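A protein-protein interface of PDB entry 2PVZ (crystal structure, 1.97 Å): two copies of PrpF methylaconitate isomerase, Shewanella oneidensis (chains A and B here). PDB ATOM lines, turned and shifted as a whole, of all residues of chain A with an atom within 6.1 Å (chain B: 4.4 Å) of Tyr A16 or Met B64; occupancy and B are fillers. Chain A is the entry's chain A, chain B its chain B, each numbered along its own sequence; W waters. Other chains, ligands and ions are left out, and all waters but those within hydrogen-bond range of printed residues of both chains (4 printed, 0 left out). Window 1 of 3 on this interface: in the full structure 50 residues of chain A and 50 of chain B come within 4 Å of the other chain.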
ATOM      1  N   ALA A  14      -8.761  14.405 -36.274  1.00  0.00           N
ATOM      2  CA  ALA A  14      -9.674  13.347 -35.842  1.00  0.00           C
ATOM      3  C   ALA A  14     -10.199  13.618 -34.442  1.00  0.00           C
ATOM      4  O   ALA A  14      -9.578  14.350 -33.660  1.00  0.00           O
ATOM      5  CB  ALA A  14      -8.967  12.002 -35.869  1.00  0.00           C
ATOM      6  N   THR A  15     -11.333  12.995 -34.128  1.00  0.00           N
ATOM      7  CA  THR A  15     -11.907  13.037 -32.791  1.00  0.00           C
ATOM      8  C   THR A  15     -12.174  11.616 -32.295  1.00  0.00           C
ATOM      9  O   THR A  15     -12.772  10.801 -33.002  1.00  0.00           O
ATOM     10  CB  THR A  15     -13.203  13.872 -32.767  1.00  0.00           C
ATOM     11  OG1 THR A  15     -12.943  15.154 -33.349  1.00  0.00           O
ATOM     12  CG2 THR A  15     -13.684  14.080 -31.343  1.00  0.00           C
ATOM     13  N   TYR A  16     -11.701  11.328 -31.087  1.00  0.00           N
ATOM     14  CA  TYR A  16     -11.923  10.041 -30.444  1.00  0.00           C
ATOM     15  C   TYR A  16     -13.111  10.206 -29.504  1.00  0.00           C
ATOM     16  O   TYR A  16     -13.081  11.040 -28.599  1.00  0.00           O
ATOM     17  CB  TYR A  16     -10.671   9.620 -29.673  1.00  0.00           C
ATOM     18  CG  TYR A  16     -10.685   8.198 -29.153  1.00  0.00           C
ATOM     19  CD1 TYR A  16     -10.920   7.116 -30.008  1.00  0.00           C
ATOM     20  CD2 TYR A  16     -10.416   7.934 -27.815  1.00  0.00           C
ATOM     21  CE1 TYR A  16     -10.913   5.800 -29.531  1.00  0.00           C
ATOM     22  CE2 TYR A  16     -10.407   6.620 -27.322  1.00  0.00           C
ATOM     23  CZ  TYR A  16     -10.658   5.563 -28.187  1.00  0.00           C
ATOM     24  OH  TYR A  16     -10.643   4.271 -27.710  1.00  0.00           O
ATOM     25  N   MET A  17     -14.165   9.429 -29.746  1.00  0.00           N
ATOM     26  CA  MET A  17     -15.416   9.586 -29.017  1.00  0.00           C
ATOM     27  C   MET A  17     -15.953   8.274 -28.454  1.00  0.00           C
ATOM     28  O   MET A  17     -15.741   7.212 -29.030  1.00  0.00           O
ATOM     29  CB  MET A  17     -16.490  10.169 -29.943  1.00  0.00           C
ATOM     30  CG  MET A  17     -16.149  11.504 -30.577  1.00  0.00           C
ATOM     31  SD  MET A  17     -17.528  12.179 -31.532  1.00  0.00           S
ATOM     32  CE  MET A  17     -18.666  12.651 -30.227  1.00  0.00           C
ATOM     33  N   ARG A  18     -16.662   8.366 -27.332  1.00  0.00           N
ATOM     34  CA  ARG A  18     -17.556   7.291 -26.916  1.00  0.00           C
ATOM     35  C   ARG A  18     -18.946   7.604 -27.478  1.00  0.00           C
ATOM     36  O   ARG A  18     -19.420   8.738 -27.386  1.00  0.00           O
ATOM     37  CB  ARG A  18     -17.627   7.165 -25.387  1.00  0.00           C
ATOM     38  CG  ARG A  18     -18.695   6.144 -24.921  1.00  0.00           C
ATOM     39  CD  ARG A  18     -18.928   6.134 -23.399  1.00  0.00           C
ATOM     40  NE  ARG A  18     -19.579   7.350 -22.907  1.00  0.00           N
ATOM     41  CZ  ARG A  18     -20.846   7.691 -23.140  1.00  0.00           C
ATOM     42  NH1 ARG A  18     -21.639   6.909 -23.878  1.00  0.00           N
ATOM     43  NH2 ARG A  18     -21.325   8.820 -22.634  1.00  0.00           N
ATOM     44  N   LYS A  23     -16.367   2.813 -28.521  1.00  0.00           N
ATOM     45  CA  LYS A  23     -15.430   3.906 -28.817  1.00  0.00           C
ATOM     46  C   LYS A  23     -15.010   3.858 -30.276  1.00  0.00           C
ATOM     47  O   LYS A  23     -14.821   2.778 -30.840  1.00  0.00           O
ATOM     48  CB  LYS A  23     -14.193   3.840 -27.917  1.00  0.00           C
ATOM     49  CG  LYS A  23     -14.509   3.982 -26.430  1.00  0.00           C
ATOM     50  CD  LYS A  23     -13.261   4.293 -25.595  1.00  0.00           C
ATOM     51  CE  LYS A  23     -12.435   3.049 -25.303  1.00  0.00           C
ATOM     52  NZ  LYS A  23     -11.242   3.379 -24.457  1.00  0.00           N
ATOM     53  N   GLY A  24     -14.858   5.030 -30.887  1.00  0.00           N
ATOM     54  CA  GLY A  24     -14.475   5.111 -32.299  1.00  0.00           C
ATOM     55  C   GLY A  24     -13.659   6.347 -32.617  1.00  0.00           C
ATOM     56  O   GLY A  24     -13.745   7.364 -31.920  1.00  0.00           O
ATOM     57  N   VAL A  25     -12.861   6.251 -33.680  1.00  0.00           N
ATOM     58  CA  VAL A  25     -12.121   7.394 -34.210  1.00  0.00           C
ATOM     59  C   VAL A  25     -12.930   7.993 -35.367  1.00  0.00           C
ATOM     60  O   VAL A  25     -13.219   7.308 -36.357  1.00  0.00           O
ATOM     61  CB  VAL A  25     -10.701   6.995 -34.695  1.00  0.00           C
ATOM     62  CG1 VAL A  25      -9.920   8.231 -35.153  1.00  0.00           C
ATOM     63  CG2 VAL A  25      -9.936   6.259 -33.593  1.00  0.00           C
ATOM     64  N   PHE A  26     -13.300   9.261 -35.220  1.00  0.00           N
ATOM     65  CA  PHE A  26     -14.168   9.955 -36.175  1.00  0.00           C
ATOM     66  C   PHE A  26     -13.355  10.931 -37.009  1.00  0.00           C
ATOM     67  O   PHE A  26     -12.492  11.633 -36.473  1.00  0.00           O
ATOM     68  CB  PHE A  26     -15.248  10.751 -35.435  1.00  0.00           C
ATOM     69  CG  PHE A  26     -16.306   9.903 -34.780  1.00  0.00           C
ATOM     70  CD1 PHE A  26     -17.627   9.980 -35.205  1.00  0.00           C
ATOM     71  CD2 PHE A  26     -15.986   9.048 -33.727  1.00  0.00           C
ATOM     72  CE1 PHE A  26     -18.619   9.210 -34.603  1.00  0.00           C
ATOM     73  CE2 PHE A  26     -16.972   8.277 -33.110  1.00  0.00           C
ATOM     74  CZ  PHE A  26     -18.288   8.353 -33.554  1.00  0.00           C
ATOM     75  N   MET A  64      -4.916   3.229 -32.031  1.00  0.00           N
ATOM     76  CA  MET A  64      -6.030   3.781 -31.256  1.00  0.00           C
ATOM     77  C   MET A  64      -7.028   2.735 -30.769  1.00  0.00           C
ATOM     78  O   MET A  64      -7.872   3.036 -29.920  1.00  0.00           O
ATOM     79  CB  MET A  64      -6.769   4.861 -32.061  1.00  0.00           C
ATOM     80  CG  MET A  64      -5.955   6.140 -32.321  1.00  0.00           C
ATOM     81  SD  MET A  64      -5.266   6.886 -30.822  1.00  0.00           S
ATOM     82  CE  MET A  64      -6.754   7.329 -29.917  1.00  0.00           C
ATOM     83  N   GLY A  65      -6.933   1.516 -31.299  1.00  0.00           N
ATOM     84  CA  GLY A  65      -7.843   0.434 -30.918  1.00  0.00           C
ATOM     85  C   GLY A  65      -7.706  -0.025 -29.470  1.00  0.00           C
ATOM     86  O   GLY A  65      -6.667   0.183 -28.837  1.00  0.00           O
ATOM     87  N   GLY A  66      -8.762  -0.643 -28.947  1.00  0.00           N
ATOM     88  CA  GLY A  66      -8.753  -1.194 -27.592  1.00  0.00           C
ATOM     89  C   GLY A  66      -8.751  -2.714 -27.559  1.00  0.00           C
ATOM     90  O   GLY A  66      -8.989  -3.310 -26.508  1.00  0.00           O
ATOM     91  N   THR A  71     -14.242  -1.449 -29.475  1.00  0.00           N
ATOM     92  CA  THR A  71     -13.192  -0.431 -29.459  1.00  0.00           C
ATOM     93  C   THR A  71     -12.243  -0.473 -30.676  1.00  0.00           C
ATOM     94  O   THR A  71     -11.143   0.070 -30.617  1.00  0.00           O
ATOM     95  CB  THR A  71     -12.346  -0.502 -28.145  1.00  0.00           C
ATOM     96  OG1 THR A  71     -11.723  -1.784 -28.043  1.00  0.00           O
ATOM     97  CG2 THR A  71     -13.209  -0.252 -26.888  1.00  0.00           C
ATOM     98  N   ARG A 385     -19.813  11.313 -25.919  1.00  0.00           N
ATOM     99  CA  ARG A 385     -18.902  12.378 -25.519  1.00  0.00           C
ATOM    100  C   ARG A 385     -17.554  12.258 -26.205  1.00  0.00           C
ATOM    101  O   ARG A 385     -17.096  11.154 -26.540  1.00  0.00           O
ATOM    102  CB  ARG A 385     -18.728  12.455 -23.989  1.00  0.00           C
ATOM    103  CG  ARG A 385     -18.241  11.174 -23.322  1.00  0.00           C
ATOM    104  CD  ARG A 385     -18.118  11.352 -21.795  1.00  0.00           C
ATOM    105  NE  ARG A 385     -16.925  12.107 -21.477  1.00  0.00           N
ATOM    106  CZ  ARG A 385     -15.767  11.582 -21.083  1.00  0.00           C
ATOM    107  NH1 ARG A 385     -15.624  10.274 -20.913  1.00  0.00           N
ATOM    108  NH2 ARG A 385     -14.744  12.388 -20.863  1.00  0.00           N
ATOM    109  N   VAL A 386     -16.926  13.410 -26.396  1.00  0.00           N
ATOM    110  CA  VAL A 386     -15.565  13.485 -26.913  1.00  0.00           C
ATOM    111  C   VAL A 386     -14.597  13.079 -25.804  1.00  0.00           C
ATOM    112  O   VAL A 386     -14.690  13.573 -24.671  1.00  0.00           O
ATOM    113  CB  VAL A 386     -15.247  14.919 -27.405  1.00  0.00           C
ATOM    114  CG1 VAL A 386     -13.762  15.078 -27.753  1.00  0.00           C
ATOM    115  CG2 VAL A 386     -16.141  15.288 -28.600  1.00  0.00           C
ATOM    116  N   LEU A 387     -13.671  12.186 -26.145  1.00  0.00           N
ATOM    117  CA  LEU A 387     -12.645  11.716 -25.213  1.00  0.00           C
ATOM    118  C   LEU A 387     -11.320  12.415 -25.494  1.00  0.00           C
ATOM    119  O   LEU A 387     -10.611  12.825 -24.573  1.00  0.00           O
ATOM    120  CB  LEU A 387     -12.473  10.197 -25.345  1.00  0.00           C
ATOM    121  CG  LEU A 387     -13.723   9.328 -25.158  1.00  0.00           C
ATOM    122  CD1 LEU A 387     -13.383   7.849 -25.304  1.00  0.00           C
ATOM    123  CD2 LEU A 387     -14.340   9.589 -23.792  1.00  0.00           C
ATOM    124  N   MET A 388     -10.995  12.542 -26.777  1.00  0.00           N
ATOM    125  CA  MET A 388      -9.795  13.259 -27.209  1.00  0.00           C
ATOM    126  C   MET A 388     -10.038  13.841 -28.591  1.00  0.00           C
ATOM    127  O   MET A 388     -10.723  13.232 -29.430  1.00  0.00           O
ATOM    128  CB  MET A 388      -8.573  12.320 -27.218  1.00  0.00           C
ATOM    129  CG  MET A 388      -7.231  13.039 -27.351  1.00  0.00           C
ATOM    130  SD  MET A 388      -5.808  11.988 -27.008  1.00  0.00           S
ATOM    131  CE  MET A 388      -4.497  13.219 -27.020  1.00  0.00           C
ATOM    132  N   GLU A 389      -9.492  15.030 -28.819  1.00  0.00           N
ATOM    133  CA  GLU A 389      -9.634  15.704 -30.102  1.00  0.00           C
ATOM    134  C   GLU A 389      -8.292  16.284 -30.504  1.00  0.00           C
ATOM    135  O   GLU A 389      -7.530  16.739 -29.646  1.00  0.00           O
ATOM    136  CB  GLU A 389     -10.680  16.825 -30.016  1.00  0.00           C
ATOM    137  CG  GLU A 389     -10.297  17.939 -29.035  1.00  0.00           C
ATOM    138  CD  GLU A 389     -11.389  18.966 -28.827  1.00  0.00           C
ATOM    139  OE1 GLU A 389     -11.943  19.478 -29.823  1.00  0.00           O
ATOM    140  OE2 GLU A 389     -11.677  19.265 -27.650  1.00  0.00           O
ATOM    141  N   TYR B  16      -1.257  11.152 -26.486  1.00  0.00           N
ATOM    142  CA  TYR B  16      -1.440   9.725 -26.272  1.00  0.00           C
ATOM    143  C   TYR B  16      -0.338   9.005 -27.048  1.00  0.00           C
ATOM    144  O   TYR B  16      -0.223   9.165 -28.267  1.00  0.00           O
ATOM    145  CB  TYR B  16      -2.829   9.306 -26.764  1.00  0.00           C
ATOM    146  CG  TYR B  16      -3.246   7.882 -26.461  1.00  0.00           C
ATOM    147  CD1 TYR B  16      -3.179   7.369 -25.162  1.00  0.00           C
ATOM    148  CD2 TYR B  16      -3.764   7.064 -27.468  1.00  0.00           C
ATOM    149  CE1 TYR B  16      -3.589   6.063 -24.885  1.00  0.00           C
ATOM    150  CE2 TYR B  16      -4.183   5.763 -27.202  1.00  0.00           C
ATOM    151  CZ  TYR B  16      -4.084   5.269 -25.906  1.00  0.00           C
ATOM    152  OH  TYR B  16      -4.490   3.977 -25.631  1.00  0.00           O
ATOM    153  N   VAL B  25      -1.256   8.271 -21.461  1.00  0.00           N
ATOM    154  CA  VAL B  25      -1.614   9.669 -21.699  1.00  0.00           C
ATOM    155  C   VAL B  25      -0.592  10.567 -21.004  1.00  0.00           C
ATOM    156  O   VAL B  25      -0.406  10.489 -19.783  1.00  0.00           O
ATOM    157  CB  VAL B  25      -3.056  10.010 -21.227  1.00  0.00           C
ATOM    158  CG1 VAL B  25      -3.432  11.419 -21.661  1.00  0.00           C
ATOM    159  CG2 VAL B  25      -4.065   9.002 -21.798  1.00  0.00           C
ATOM    160  N   VAL B  50      -9.911  10.955 -17.054  1.00  0.00           N
ATOM    161  CA  VAL B  50      -9.276  10.887 -18.381  1.00  0.00           C
ATOM    162  C   VAL B  50      -9.208   9.423 -18.866  1.00  0.00           C
ATOM    163  O   VAL B  50      -9.562   9.110 -20.010  1.00  0.00           O
ATOM    164  CB  VAL B  50      -7.862  11.532 -18.379  1.00  0.00           C
ATOM    165  CG1 VAL B  50      -7.106  11.216 -19.682  1.00  0.00           C
ATOM    166  CG2 VAL B  50      -7.959  13.056 -18.171  1.00  0.00           C
ATOM    167  N   ILE B  51      -8.795   8.537 -17.964  1.00  0.00           N
ATOM    168  CA  ILE B  51      -8.608   7.116 -18.274  1.00  0.00           C
ATOM    169  C   ILE B  51      -9.927   6.329 -18.352  1.00  0.00           C
ATOM    170  O   ILE B  51     -10.030   5.336 -19.090  1.00  0.00           O
ATOM    171  CB  ILE B  51      -7.608   6.483 -17.262  1.00  0.00           C
ATOM    172  CG1 ILE B  51      -6.190   7.048 -17.495  1.00  0.00           C
ATOM    173  CG2 ILE B  51      -7.605   4.962 -17.334  1.00  0.00           C
ATOM    174  CD1 ILE B  51      -5.575   6.711 -18.888  1.00  0.00           C
ATOM    175  N   GLY B  63     -13.378   6.338 -21.330  1.00  0.00           N
ATOM    176  CA  GLY B  63     -12.113   7.041 -21.137  1.00  0.00           C
ATOM    177  C   GLY B  63     -11.039   6.577 -22.099  1.00  0.00           C
ATOM    178  O   GLY B  63     -11.308   5.776 -23.008  1.00  0.00           O
ATOM    179  N   MET B  64      -9.819   7.066 -21.872  1.00  0.00           N
ATOM    180  CA  MET B  64      -8.671   6.786 -22.733  1.00  0.00           C
ATOM    181  C   MET B  64      -8.027   5.433 -22.466  1.00  0.00           C
ATOM    182  O   MET B  64      -7.170   4.990 -23.236  1.00  0.00           O
ATOM    183  CB  MET B  64      -7.614   7.896 -22.601  1.00  0.00           C
ATOM    184  CG  MET B  64      -8.037   9.250 -23.168  1.00  0.00           C
ATOM    185  SD  MET B  64      -8.637   9.189 -24.877  1.00  0.00           S
ATOM    186  CE  MET B  64      -7.180   8.581 -25.727  1.00  0.00           C
ATOM    187  N   GLY B  65      -8.421   4.778 -21.373  1.00  0.00           N
ATOM    188  CA  GLY B  65      -7.820   3.503 -21.012  1.00  0.00           C
ATOM    189  C   GLY B  65      -8.191   2.386 -21.974  1.00  0.00           C
ATOM    190  O   GLY B  65      -9.167   2.493 -22.719  1.00  0.00           O
ATOM    191  N   GLY B  66      -7.405   1.314 -21.958  1.00  0.00           N
ATOM    192  CA  GLY B  66      -7.691   0.135 -22.769  1.00  0.00           C
ATOM    193  C   GLY B  66      -8.084  -1.083 -21.947  1.00  0.00           C
ATOM    194  O   GLY B  66      -8.092  -2.202 -22.465  1.00  0.00           O
ATOM    195  N   MET B 388      -1.938   9.955 -30.797  1.00  0.00           N
ATOM    196  CA  MET B 388      -2.876  11.065 -30.895  1.00  0.00           C
ATOM    197  C   MET B 388      -2.372  12.218 -30.047  1.00  0.00           C
ATOM    198  O   MET B 388      -1.778  12.012 -28.988  1.00  0.00           O
ATOM    199  CB  MET B 388      -4.294  10.660 -30.460  1.00  0.00           C
ATOM    200  CG  MET B 388      -5.379  11.675 -30.879  1.00  0.00           C
ATOM    201  SD  MET B 388      -7.067  11.062 -30.698  1.00  0.00           S
ATOM    202  CE  MET B 388      -7.972  12.369 -31.525  1.00  0.00           C
ATOM    203  N   VAL B 392      -7.488  16.127 -24.308  1.00  0.00           N
ATOM    204  CA  VAL B 392      -8.433  15.197 -23.702  1.00  0.00           C
ATOM    205  C   VAL B 392      -9.521  16.014 -23.008  1.00  0.00           C
ATOM    206  O   VAL B 392      -9.284  17.158 -22.601  1.00  0.00           O
ATOM    207  CB  VAL B 392      -7.756  14.200 -22.706  1.00  0.00           C
ATOM    208  CG1 VAL B 392      -6.860  13.217 -23.461  1.00  0.00           C
ATOM    209  CG2 VAL B 392      -6.965  14.940 -21.613  1.00  0.00           C
HETATM  210  O   HOH W   1     -11.145   0.366 -23.668  1.00  0.00           O
HETATM  211  O   HOH W   2     -12.459  10.511 -20.514  1.00  0.00           O
HETATM  212  O   HOH W   3     -10.280  -2.075 -24.347  1.00  0.00           O
HETATM  213  O   HOH W   4      -6.732  -2.848 -24.640  1.00  0.00           O
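The side-chain amino group of Lys A23 lies within hydrogen-bond range of the backbone carbonyl oxygen of Gly B63 (2.8 Å). The backbone carbonyl oxygen (O) of Gly B65 sits at hydrogen-bond distance from the side-chain amino group (NZ) of Lys A23 (2.8 Å).
The side-chain hydroxyl of Tyr A16 lies close to the side-chain amino group of Lys A23, 3.4 Å away. The backbone NH of Leu A387 lies within hydrogen-bond range of the backbone carbonyl oxygen of Tyr A16 (2.8 Å). N of Tyr A16 lies within hydrogen-bond range of O of Met A388 (2.7 Å). The backbone NH of Tyr B16 lies within hydrogen-bond range of the backbone carbonyl oxygen of Met B388. The backbone carbonyl oxygen (O) of Ile B51 lies within hydrogen-bond range of the backbone NH (N) of Met B64, 3.3 Å away. The backbone carbonyl oxygen (O) of Ile B51 is in hydrogen-bond range of the backbone NH (N) of Gly B65, at 2.8 Å.
Met B64 touches Tyr A16. Tyr A16 touches Met B388 (N to CE, 3.9 Å). Tyr B16 touches Met A64 (CD2 to SD, 3.7 Å). Met A64 touches Met B388 (CE to SD, 3.8 Å). Leu A387 touches Gly B63 (CD1 to O, 3.7 Å). CE of Met A388 touches N of Tyr B16, 3.9 Å away. CE of Met B64 touches SD of Met A388, 3.9 Å away. O of Met A388 touches CE of Met B388, 3.6 Å away. CG1 of Val B392 touches SD of Met A388 (3.9 Å). Glu A389 touches Met B388 (CA to CE, 3.99 Å).
Of chain B, only Met B64 (3.7 Å) and Met B388 (3.9 Å) come within 4 Å of Tyr A16. Of the printed residues of chain B, Lys A23 touches Gly B63 and Gly B65. Of the printed residues of chain B, Ala A14 touches Met B388. Phe A26 touches none of the printed residues of chain B. Gly A65 touches none of the printed residues of chain B. The nearest printed residue of chain B that does not touch Tyr A16 is Gly B63 (4.5 Å). The nearest printed residue of chain A that does not touch Met B64 is Lys A23 (4.3 Å).
Hydrophobic or aromatic side chains of chain B within 4 Å of the printed part of chain A: Tyr B16, Met B64, Met B388 and Val B392. Along chain B the printed residues that touch a printed residue of chain A span positions 16 to 392. Of the 18 printed residues of chain A, 7 touch a printed residue of chain B. Printed residues of chain A that touch a printed residue of chain B: Ala A14, Tyr A16, Lys A23, Met A64, Leu A387, Met A388 and Glu A389. Along chain A the printed residues that touch a printed residue of chain B span positions 14 to 389. Among the printed residues, no Asp or Glu carboxylate lies within 4 Å of a Lys or Arg side-chain nitrogen of the other chain.
Tyr A16 touches Met B64, and with the chains exchanged Met A64 touches Tyr B16. Tyr A16 touches Met B388, and with the chains exchanged Met A388 touches Tyr B16. Met A64 touches Met B388, and with the chains exchanged Met A388 touches Met B64. Met A388 touches its own counterpart, Met B388. Positions printed for both chains: 16, 25, 64, 65, 66 and 388. Of the 15 pairs that touch across the chains among the printed residues, 7 have their exchanged pair printed and touching as well.
Water W4 lies within hydrogen-bond range of the backbone carbonyl oxygen of Gly B66 (2.6 Å) and the backbone carbonyl oxygen of Gly A66 (3.0 Å). Water W3 bridges the backbone carbonyl oxygen (O) of Gly A66 and the backbone carbonyl oxygen (O) of Gly B66. Water W2 bridges the guanidinium group of Arg A385 (3.0 Å) and the backbone carbonyl oxygen of Val B50 (3.3 Å). Water W1 bridges the backbone carbonyl oxygen (O) of Gly B65 (3.1 Å) and the side-chain amino group (NZ) of Lys A23 (3.1 Å).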
